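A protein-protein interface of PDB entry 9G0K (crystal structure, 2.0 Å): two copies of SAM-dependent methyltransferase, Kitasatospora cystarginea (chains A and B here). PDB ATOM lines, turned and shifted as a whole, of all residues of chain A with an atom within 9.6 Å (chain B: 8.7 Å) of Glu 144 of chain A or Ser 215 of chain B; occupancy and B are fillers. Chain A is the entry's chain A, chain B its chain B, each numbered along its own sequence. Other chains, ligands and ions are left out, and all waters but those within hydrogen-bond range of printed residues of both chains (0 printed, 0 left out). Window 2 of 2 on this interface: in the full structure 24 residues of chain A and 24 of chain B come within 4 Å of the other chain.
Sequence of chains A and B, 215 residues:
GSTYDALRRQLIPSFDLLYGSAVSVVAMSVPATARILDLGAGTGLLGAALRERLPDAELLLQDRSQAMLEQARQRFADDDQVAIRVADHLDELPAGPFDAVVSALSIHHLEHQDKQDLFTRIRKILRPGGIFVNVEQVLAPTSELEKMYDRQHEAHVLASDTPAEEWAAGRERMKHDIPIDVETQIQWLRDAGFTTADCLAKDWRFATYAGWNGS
The side-chain hydroxyl (OG) of Ser 143 of chain A is in hydrogen-bond range of the side-chain carboxylate (OE1) of Glu 144 of chain A, 3.1 Å away. OG of Ser 29 of chain B sits at hydrogen-bond distance from NE1 of Trp 212 of chain B, at 3.0 Å. The backbone NH (N) of Thr 195 of chain B lies within hydrogen-bond range of the backbone carbonyl oxygen (O) of Trp 212 of chain B (2.9 Å). The backbone NH of Ser 215 of chain B lies within hydrogen-bond range of the side-chain hydroxyl of Thr 195 of chain B (3.3 Å). The backbone carbonyl oxygen of Thr 196 of chain B lies within hydrogen-bond range of the backbone NH of Trp 212 of chain B. OG1 of Thr 196 of chain B lies within hydrogen-bond range of O of Ser 215 of chain B (2.9 Å).
OG1 of Thr 196 of chain B touches CG2 of Thr 142 of chain A, at 3.7 Å. Ser 215 of chain B touches Glu 144 of chain A. Trp 212 of chain B touches Leu 145 of chain A (CH2 to CD2, 3.9 Å). Met 28 of chain B touches Met 148 of chain A (O to CE, 3.7 Å). CE of Met 148 of chain A touches OG of Ser 29 of chain B (3.8 Å). Met 28 of chain B touches Trp 204 of chain A (CE to CH2, 3.5 Å).
Of the printed residues of chain B, Thr 142 of chain A touches Thr 196. No residue of chain B comes within 4 Å of Ser 143 of chain A. Of the printed residues of chain B, Glu 144 of chain A touches Ser 215. Asp 150 of chain A touches none of the printed residues of chain B. Printed residues of chain B within 4 Å of Trp 204 of chain A: Met 28. Printed residues of chain A within 4 Å of Met 28 of chain B: Met 148 and Trp 204. No residue of chain A comes within 4 Å of Thr 195 of chain B. Ala 197 of chain B touches none of the printed residues of chain A. No residue of chain A comes within 4 Å of Gly 214 of chain B. Of the printed residues of chain A, Ser 215 of chain B touches Glu 144 (3.7 Å). The nearest residue of chain B that does not touch Glu 144 of chain A is Thr 196 of chain B (5.8 Å).
No position is printed for both chains. Of the 6 pairs that touch across the chains among the printed residues, none has its exchanged pair printed and touching as well.
Hydrophobic or aromatic side chains of chain B that line the printed part of chain A: Met 28 and Trp 212. Of the 15 printed residues of chain A, 5 touch a printed residue of chain B. Printed residues of chain A that touch a printed residue of chain B: Thr 142, Glu 144, Leu 145, Met 148 and Trp 204. Among the printed residues, no Asp or Glu carboxylate lies within 4 Å of a Lys or Arg side-chain nitrogen of the other chain.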
ATOM      1  N   LEU A 139      25.963   2.978  38.280  1.00  0.00           N
ATOM      2  CA  LEU A 139      24.999   3.775  37.477  1.00  0.00           C
ATOM      3  C   LEU A 139      25.812   4.618  36.488  1.00  0.00           C
ATOM      4  O   LEU A 139      26.836   5.120  36.893  1.00  0.00           O
ATOM      5  CB  LEU A 139      24.220   4.671  38.450  1.00  0.00           C
ATOM      6  CG  LEU A 139      22.814   5.133  38.065  1.00  0.00           C
ATOM      7  CD1 LEU A 139      21.923   3.926  37.908  1.00  0.00           C
ATOM      8  CD2 LEU A 139      22.174   6.090  39.110  1.00  0.00           C
ATOM      9  N   ALA A 140      25.395   4.754  35.232  1.00  0.00           N
ATOM     10  CA  ALA A 140      25.804   5.852  34.318  1.00  0.00           C
ATOM     11  C   ALA A 140      25.543   7.229  34.941  1.00  0.00           C
ATOM     12  O   ALA A 140      24.639   7.397  35.779  1.00  0.00           O
ATOM     13  CB  ALA A 140      25.015   5.701  33.051  1.00  0.00           C
ATOM     14  N   PRO A 141      26.311   8.268  34.535  1.00  0.00           N
ATOM     15  CA  PRO A 141      26.112   9.611  35.083  1.00  0.00           C
ATOM     16  C   PRO A 141      24.882  10.408  34.608  1.00  0.00           C
ATOM     17  O   PRO A 141      24.666  11.412  35.211  1.00  0.00           O
ATOM     18  CB  PRO A 141      27.388  10.364  34.684  1.00  0.00           C
ATOM     19  CG  PRO A 141      27.906   9.624  33.458  1.00  0.00           C
ATOM     20  CD  PRO A 141      27.462   8.189  33.631  1.00  0.00           C
ATOM     21  N   THR A 142      24.128   9.957  33.599  1.00  0.00           N
ATOM     22  CA  THR A 142      22.880  10.590  33.079  1.00  0.00           C
ATOM     23  C   THR A 142      21.889   9.498  32.681  1.00  0.00           C
ATOM     24  O   THR A 142      22.303   8.398  32.319  1.00  0.00           O
ATOM     25  CB  THR A 142      23.099  11.504  31.856  1.00  0.00           C
ATOM     26  OG1 THR A 142      23.366  10.649  30.727  1.00  0.00           O
ATOM     27  CG2 THR A 142      24.163  12.560  32.084  1.00  0.00           C
ATOM     28  N   SER A 143      20.607   9.823  32.706  1.00  0.00           N
ATOM     29  CA  SER A 143      19.526   8.842  32.447  1.00  0.00           C
ATOM     30  C   SER A 143      19.628   8.414  30.993  1.00  0.00           C
ATOM     31  O   SER A 143      19.313   7.267  30.715  1.00  0.00           O
ATOM     32  CB  SER A 143      18.138   9.372  32.834  1.00  0.00           C
ATOM     33  OG  SER A 143      17.958  10.672  32.348  1.00  0.00           O
ATOM     34  N   GLU A 144      20.089   9.286  30.105  1.00  0.00           N
ATOM     35  CA  GLU A 144      20.292   8.875  28.686  1.00  0.00           C
ATOM     36  C   GLU A 144      21.347   7.761  28.623  1.00  0.00           C
ATOM     37  O   GLU A 144      21.092   6.744  27.960  1.00  0.00           O
ATOM     38  CB  GLU A 144      20.694  10.085  27.846  1.00  0.00           C
ATOM     39  CG  GLU A 144      19.722  11.249  27.947  1.00  0.00           C
ATOM     40  CD  GLU A 144      19.964  12.203  29.106  1.00  0.00           C
ATOM     41  OE1 GLU A 144      19.937  11.751  30.265  1.00  0.00           O
ATOM     42  OE2 GLU A 144      20.188  13.400  28.843  1.00  0.00           O
ATOM     43  N   LEU A 145      22.464   7.940  29.318  1.00  0.00           N
ATOM     44  CA  LEU A 145      23.575   6.939  29.340  1.00  0.00           C
ATOM     45  C   LEU A 145      23.161   5.658  30.078  1.00  0.00           C
ATOM     46  O   LEU A 145      23.557   4.568  29.664  1.00  0.00           O
ATOM     47  CB  LEU A 145      24.790   7.568  30.009  1.00  0.00           C
ATOM     48  CG  LEU A 145      25.936   8.004  29.118  1.00  0.00           C
ATOM     49  CD1 LEU A 145      27.065   8.564  29.948  1.00  0.00           C
ATOM     50  CD2 LEU A 145      26.471   6.864  28.348  1.00  0.00           C
ATOM     51  N   GLU A 146      22.411   5.773  31.159  1.00  0.00           N
ATOM     52  CA  GLU A 146      21.913   4.591  31.903  1.00  0.00           C
ATOM     53  C   GLU A 146      21.163   3.647  30.956  1.00  0.00           C
ATOM     54  O   GLU A 146      21.330   2.404  31.103  1.00  0.00           O
ATOM     55  CB  GLU A 146      20.976   5.036  33.033  1.00  0.00           C
ATOM     56  CG  GLU A 146      20.481   3.861  33.877  1.00  0.00           C
ATOM     57  CD  GLU A 146      21.538   2.864  34.368  1.00  0.00           C
ATOM     58  OE1 GLU A 146      22.704   3.270  34.650  1.00  0.00           O
ATOM     59  OE2 GLU A 146      21.207   1.652  34.431  1.00  0.00           O
ATOM     60  N   LYS A 147      20.383   4.202  30.012  1.00  0.00           N
ATOM     61  CA  LYS A 147      19.645   3.402  28.992  1.00  0.00           C
ATOM     62  C   LYS A 147      20.649   2.681  28.062  1.00  0.00           C
ATOM     63  O   LYS A 147      20.437   1.461  27.748  1.00  0.00           O
ATOM     64  CB  LYS A 147      18.657   4.288  28.231  1.00  0.00           C
ATOM     65  CG  LYS A 147      17.897   3.590  27.111  1.00  0.00           C
ATOM     66  CD  LYS A 147      17.087   2.439  27.647  1.00  0.00           C
ATOM     67  CE  LYS A 147      16.385   1.558  26.637  1.00  0.00           C
ATOM     68  NZ  LYS A 147      16.067   0.236  27.248  1.00  0.00           N
ATOM     69  N   MET A 148      21.735   3.355  27.659  1.00  0.00           N
ATOM     70  CA  MET A 148      22.822   2.735  26.843  1.00  0.00           C
ATOM     71  C   MET A 148      23.533   1.620  27.639  1.00  0.00           C
ATOM     72  O   MET A 148      23.770   0.508  27.075  1.00  0.00           O
ATOM     73  CB  MET A 148      23.842   3.791  26.400  1.00  0.00           C
ATOM     74  CG  MET A 148      23.239   4.929  25.574  1.00  0.00           C
ATOM     75  SD  MET A 148      24.556   5.889  24.850  1.00  0.00           S
ATOM     76  CE  MET A 148      23.667   7.232  24.064  1.00  0.00           C
ATOM     77  N   TYR A 149      23.886   1.881  28.876  1.00  0.00           N
ATOM     78  CA  TYR A 149      24.456   0.881  29.807  1.00  0.00           C
ATOM     79  C   TYR A 149      23.580  -0.360  29.828  1.00  0.00           C
ATOM     80  O   TYR A 149      24.110  -1.462  29.829  1.00  0.00           O
ATOM     81  CB  TYR A 149      24.590   1.407  31.247  1.00  0.00           C
ATOM     82  CG  TYR A 149      25.815   2.241  31.517  1.00  0.00           C
ATOM     83  CD1 TYR A 149      26.482   2.100  32.710  1.00  0.00           C
ATOM     84  CD2 TYR A 149      26.277   3.202  30.631  1.00  0.00           C
ATOM     85  CE1 TYR A 149      27.573   2.874  33.011  1.00  0.00           C
ATOM     86  CE2 TYR A 149      27.327   4.032  30.955  1.00  0.00           C
ATOM     87  CZ  TYR A 149      28.013   3.820  32.122  1.00  0.00           C
ATOM     88  OH  TYR A 149      29.040   4.588  32.558  1.00  0.00           O
ATOM     89  N   ASP A 150      22.274  -0.163  29.883  1.00  0.00           N
ATOM     90  CA  ASP A 150      21.282  -1.249  30.036  1.00  0.00           C
ATOM     91  C   ASP A 150      21.252  -2.047  28.731  1.00  0.00           C
ATOM     92  O   ASP A 150      21.273  -3.294  28.803  1.00  0.00           O
ATOM     93  CB  ASP A 150      19.927  -0.655  30.407  1.00  0.00           C
ATOM     94  CG  ASP A 150      18.964  -1.687  30.947  1.00  0.00           C
ATOM     95  OD1 ASP A 150      18.972  -1.917  32.214  1.00  0.00           O
ATOM     96  OD2 ASP A 150      18.191  -2.207  30.135  1.00  0.00           O
ATOM     97  N   ARG A 151      21.228  -1.387  27.571  1.00  0.00           N
ATOM     98  CA  ARG A 151      21.260  -2.133  26.271  1.00  0.00           C
ATOM     99  C   ARG A 151      22.559  -2.945  26.155  1.00  0.00           C
ATOM    100  O   ARG A 151      22.529  -4.041  25.528  1.00  0.00           O
ATOM    101  CB  ARG A 151      21.140  -1.196  25.070  1.00  0.00           C
ATOM    102  CG  ARG A 151      19.806  -0.483  25.000  1.00  0.00           C
ATOM    103  CD  ARG A 151      19.741   0.465  23.825  1.00  0.00           C
ATOM    104  NE  ARG A 151      18.349   0.816  23.527  1.00  0.00           N
ATOM    105  CZ  ARG A 151      17.589   0.241  22.593  1.00  0.00           C
ATOM    106  NH1 ARG A 151      18.062  -0.746  21.838  1.00  0.00           N
ATOM    107  NH2 ARG A 151      16.373   0.697  22.375  1.00  0.00           N
ATOM    108  N   TRP A 204      31.098  -0.772  30.897  1.00  0.00           N
ATOM    109  CA  TRP A 204      29.844   0.013  31.029  1.00  0.00           C
ATOM    110  C   TRP A 204      29.299  -0.043  32.467  1.00  0.00           C
ATOM    111  O   TRP A 204      29.854   0.653  33.323  1.00  0.00           O
ATOM    112  CB  TRP A 204      28.818  -0.410  29.967  1.00  0.00           C
ATOM    113  CG  TRP A 204      29.276  -0.197  28.554  1.00  0.00           C
ATOM    114  CD1 TRP A 204      30.259  -0.878  27.897  1.00  0.00           C
ATOM    115  CD2 TRP A 204      28.767   0.764  27.611  1.00  0.00           C
ATOM    116  NE1 TRP A 204      30.399  -0.415  26.617  1.00  0.00           N
ATOM    117  CE2 TRP A 204      29.499   0.595  26.413  1.00  0.00           C
ATOM    118  CE3 TRP A 204      27.772   1.746  27.660  1.00  0.00           C
ATOM    119  CZ2 TRP A 204      29.261   1.370  25.281  1.00  0.00           C
ATOM    120  CZ3 TRP A 204      27.541   2.514  26.541  1.00  0.00           C
ATOM    121  CH2 TRP A 204      28.276   2.325  25.369  1.00  0.00           C
ATOM    122  N   ARG A 205      28.288  -0.882  32.720  1.00  0.00           N
ATOM    123  CA  ARG A 205      27.614  -1.002  34.047  1.00  0.00           C
ATOM    124  C   ARG A 205      28.498  -1.671  35.112  1.00  0.00           C
ATOM    125  O   ARG A 205      28.162  -1.541  36.304  1.00  0.00           O
ATOM    126  CB  ARG A 205      26.285  -1.751  33.893  1.00  0.00           C
ATOM    127  CG  ARG A 205      25.506  -1.925  35.190  1.00  0.00           C
ATOM    128  CD  ARG A 205      24.129  -2.527  34.984  1.00  0.00           C
ATOM    129  NE  ARG A 205      23.132  -1.522  34.653  1.00  0.00           N
ATOM    130  CZ  ARG A 205      22.005  -1.758  33.994  1.00  0.00           C
ATOM    131  NH1 ARG A 205      21.714  -2.981  33.591  1.00  0.00           N
ATOM    132  NH2 ARG A 205      21.172  -0.767  33.739  1.00  0.00           N
ATOM    133  N   MET B  28      24.601   4.093  18.991  1.00  0.00           N
ATOM    134  CA  MET B  28      23.395   4.478  19.794  1.00  0.00           C
ATOM    135  C   MET B  28      23.281   6.011  19.892  1.00  0.00           C
ATOM    136  O   MET B  28      22.430   6.452  20.613  1.00  0.00           O
ATOM    137  CB  MET B  28      23.414   3.910  21.220  1.00  0.00           C
ATOM    138  CG  MET B  28      23.491   2.400  21.315  1.00  0.00           C
ATOM    139  SD  MET B  28      23.642   1.797  23.057  1.00  0.00           S
ATOM    140  CE  MET B  28      25.388   1.983  23.453  1.00  0.00           C
ATOM    141  N   SER B  29      24.168   6.778  19.255  1.00  0.00           N
ATOM    142  CA  SER B  29      24.299   8.239  19.455  1.00  0.00           C
ATOM    143  C   SER B  29      23.895   8.969  18.182  1.00  0.00           C
ATOM    144  O   SER B  29      23.404  10.097  18.300  1.00  0.00           O
ATOM    145  CB  SER B  29      25.685   8.631  19.863  1.00  0.00           C
ATOM    146  OG  SER B  29      25.911   8.396  21.257  1.00  0.00           O
ATOM    147  N   ARG B 127      27.917  18.520  15.194  1.00  0.00           N
ATOM    148  CA  ARG B 127      26.515  19.020  15.216  1.00  0.00           C
ATOM    149  C   ARG B 127      26.094  19.054  16.681  1.00  0.00           C
ATOM    150  O   ARG B 127      26.755  18.442  17.525  1.00  0.00           O
ATOM    151  CB  ARG B 127      25.566  18.092  14.441  1.00  0.00           C
ATOM    152  CG  ARG B 127      25.641  18.205  12.935  1.00  0.00           C
ATOM    153  CD  ARG B 127      24.802  17.197  12.131  1.00  0.00           C
ATOM    154  NE  ARG B 127      25.205  16.849  10.727  1.00  0.00           N
ATOM    155  CZ  ARG B 127      25.037  17.650   9.671  1.00  0.00           C
ATOM    156  NH1 ARG B 127      24.538  18.872   9.832  1.00  0.00           N
ATOM    157  NH2 ARG B 127      25.363  17.226   8.457  1.00  0.00           N
ATOM    158  N   PRO B 128      25.039  19.796  17.055  1.00  0.00           N
ATOM    159  CA  PRO B 128      24.440  19.712  18.408  1.00  0.00           C
ATOM    160  C   PRO B 128      23.973  18.304  18.805  1.00  0.00           C
ATOM    161  O   PRO B 128      23.192  17.784  18.095  1.00  0.00           O
ATOM    162  CB  PRO B 128      23.197  20.600  18.310  1.00  0.00           C
ATOM    163  CG  PRO B 128      23.568  21.624  17.262  1.00  0.00           C
ATOM    164  CD  PRO B 128      24.429  20.856  16.249  1.00  0.00           C
ATOM    165  N   GLY B 129      24.416  17.761  19.938  1.00  0.00           N
ATOM    166  CA  GLY B 129      24.188  16.354  20.330  1.00  0.00           C
ATOM    167  C   GLY B 129      25.172  15.395  19.672  1.00  0.00           C
ATOM    168  O   GLY B 129      25.036  14.208  19.879  1.00  0.00           O
ATOM    169  N   GLY B 130      26.144  15.887  18.910  1.00  0.00           N
ATOM    170  CA  GLY B 130      27.200  15.053  18.293  1.00  0.00           C
ATOM    171  C   GLY B 130      28.092  14.453  19.358  1.00  0.00           C
ATOM    172  O   GLY B 130      28.067  14.932  20.479  1.00  0.00           O
ATOM    173  N   ILE B 131      28.859  13.424  18.983  1.00  0.00           N
ATOM    174  CA  ILE B 131      29.641  12.688  20.015  1.00  0.00           C
ATOM    175  C   ILE B 131      31.118  12.510  19.658  1.00  0.00           C
ATOM    176  O   ILE B 131      31.410  12.090  18.519  1.00  0.00           O
ATOM    177  CB  ILE B 131      28.989  11.317  20.294  1.00  0.00           C
ATOM    178  CG1 ILE B 131      29.759  10.529  21.357  1.00  0.00           C
ATOM    179  CG2 ILE B 131      28.831  10.519  19.009  1.00  0.00           C
ATOM    180  CD1 ILE B 131      29.230   9.134  21.583  1.00  0.00           C
ATOM    181  N   GLY B 193      33.503  22.092  26.775  1.00  0.00           N
ATOM    182  CA  GLY B 193      32.080  22.464  26.717  1.00  0.00           C
ATOM    183  C   GLY B 193      31.178  21.282  26.370  1.00  0.00           C
ATOM    184  O   GLY B 193      30.025  21.531  26.039  1.00  0.00           O
ATOM    185  N   PHE B 194      31.663  20.041  26.342  1.00  0.00           N
ATOM    186  CA  PHE B 194      30.753  18.883  26.196  1.00  0.00           C
ATOM    187  C   PHE B 194      29.893  18.848  27.476  1.00  0.00           C
ATOM    188  O   PHE B 194      30.393  19.033  28.582  1.00  0.00           O
ATOM    189  CB  PHE B 194      31.554  17.612  25.934  1.00  0.00           C
ATOM    190  CG  PHE B 194      32.303  17.561  24.612  1.00  0.00           C
ATOM    191  CD1 PHE B 194      31.835  16.780  23.568  1.00  0.00           C
ATOM    192  CD2 PHE B 194      33.489  18.244  24.416  1.00  0.00           C
ATOM    193  CE1 PHE B 194      32.515  16.703  22.360  1.00  0.00           C
ATOM    194  CE2 PHE B 194      34.183  18.137  23.221  1.00  0.00           C
ATOM    195  CZ  PHE B 194      33.693  17.360  22.199  1.00  0.00           C
ATOM    196  N   THR B 195      28.562  18.622  27.261  1.00  0.00           N
ATOM    197  CA  THR B 195      27.596  18.614  28.395  1.00  0.00           C
ATOM    198  C   THR B 195      27.779  17.354  29.249  1.00  0.00           C
ATOM    199  O   THR B 195      27.672  17.470  30.484  1.00  0.00           O
ATOM    200  CB  THR B 195      26.174  18.749  27.843  1.00  0.00           C
ATOM    201  OG1 THR B 195      26.064  17.853  26.738  1.00  0.00           O
ATOM    202  CG2 THR B 195      25.853  20.153  27.383  1.00  0.00           C
ATOM    203  N   THR B 196      28.036  16.222  28.644  1.00  0.00           N
ATOM    204  CA  THR B 196      28.245  14.914  29.321  1.00  0.00           C
ATOM    205  C   THR B 196      29.556  14.300  28.792  1.00  0.00           C
ATOM    206  O   THR B 196      29.777  14.368  27.525  1.00  0.00           O
ATOM    207  CB  THR B 196      27.120  13.932  29.007  1.00  0.00           C
ATOM    208  OG1 THR B 196      25.880  14.443  29.448  1.00  0.00           O
ATOM    209  CG2 THR B 196      27.238  12.619  29.735  1.00  0.00           C
ATOM    210  N   ALA B 197      30.409  13.790  29.697  1.00  0.00           N
ATOM    211  CA  ALA B 197      31.607  12.981  29.381  1.00  0.00           C
ATOM    212  C   ALA B 197      31.679  11.769  30.316  1.00  0.00           C
ATOM    213  O   ALA B 197      31.334  11.916  31.504  1.00  0.00           O
ATOM    214  CB  ALA B 197      32.806  13.853  29.546  1.00  0.00           C
ATOM    215  N   GLY B 211      32.489  12.188  24.788  1.00  0.00           N
ATOM    216  CA  GLY B 211      31.666  13.309  25.270  1.00  0.00           C
ATOM    217  C   GLY B 211      30.603  13.668  24.295  1.00  0.00           C
ATOM    218  O   GLY B 211      30.734  13.277  23.123  1.00  0.00           O
ATOM    219  N   TRP B 212      29.515  14.259  24.818  1.00  0.00           N
ATOM    220  CA  TRP B 212      28.325  14.612  24.014  1.00  0.00           C
ATOM    221  C   TRP B 212      28.208  16.127  24.012  1.00  0.00           C
ATOM    222  O   TRP B 212      28.304  16.729  25.111  1.00  0.00           O
ATOM    223  CB  TRP B 212      27.056  13.952  24.579  1.00  0.00           C
ATOM    224  CG  TRP B 212      27.023  12.482  24.309  1.00  0.00           C
ATOM    225  CD1 TRP B 212      26.452  11.844  23.237  1.00  0.00           C
ATOM    226  CD2 TRP B 212      27.665  11.466  25.081  1.00  0.00           C
ATOM    227  NE1 TRP B 212      26.661  10.498  23.307  1.00  0.00           N
ATOM    228  CE2 TRP B 212      27.455  10.239  24.393  1.00  0.00           C
ATOM    229  CE3 TRP B 212      28.476  11.484  26.188  1.00  0.00           C
ATOM    230  CZ2 TRP B 212      27.924   9.012  24.866  1.00  0.00           C
ATOM    231  CZ3 TRP B 212      28.945  10.281  26.659  1.00  0.00           C
ATOM    232  CH2 TRP B 212      28.684   9.065  26.008  1.00  0.00           C
ATOM    233  N   ASN B 213      27.934  16.667  22.823  1.00  0.00           N
ATOM    234  CA  ASN B 213      27.754  18.104  22.535  1.00  0.00           C
ATOM    235  C   ASN B 213      26.273  18.523  22.677  1.00  0.00           C
ATOM    236  O   ASN B 213      25.609  18.841  21.679  1.00  0.00           O
ATOM    237  CB  ASN B 213      28.263  18.359  21.134  1.00  0.00           C
ATOM    238  CG  ASN B 213      28.373  19.817  20.813  1.00  0.00           C
ATOM    239  OD1 ASN B 213      28.572  20.659  21.677  1.00  0.00           O
ATOM    240  ND2 ASN B 213      28.173  20.118  19.565  1.00  0.00           N
ATOM    241  N   GLY B 214      25.739  18.551  23.887  1.00  0.00           N
ATOM    242  CA  GLY B 214      24.394  19.090  24.096  1.00  0.00           C
ATOM    243  C   GLY B 214      23.559  18.135  24.930  1.00  0.00           C
ATOM    244  O   GLY B 214      22.807  18.635  25.830  1.00  0.00           O
ATOM    245  N   SER B 215      23.727  16.819  24.698  1.00  0.00           N
ATOM    246  CA  SER B 215      23.045  15.717  25.447  1.00  0.00           C
ATOM    247  C   SER B 215      23.849  15.283  26.703  1.00  0.00           C
ATOM    248  O   SER B 215      24.950  15.785  26.998  1.00  0.00           O
ATOM    249  CB  SER B 215      22.756  14.543  24.505  1.00  0.00           C
ATOM    250  OG  SER B 215      23.950  13.943  23.995  1.00  0.00           O
ATOM    251  OXT SER B 215      23.459  14.407  27.531  1.00  0.00           O
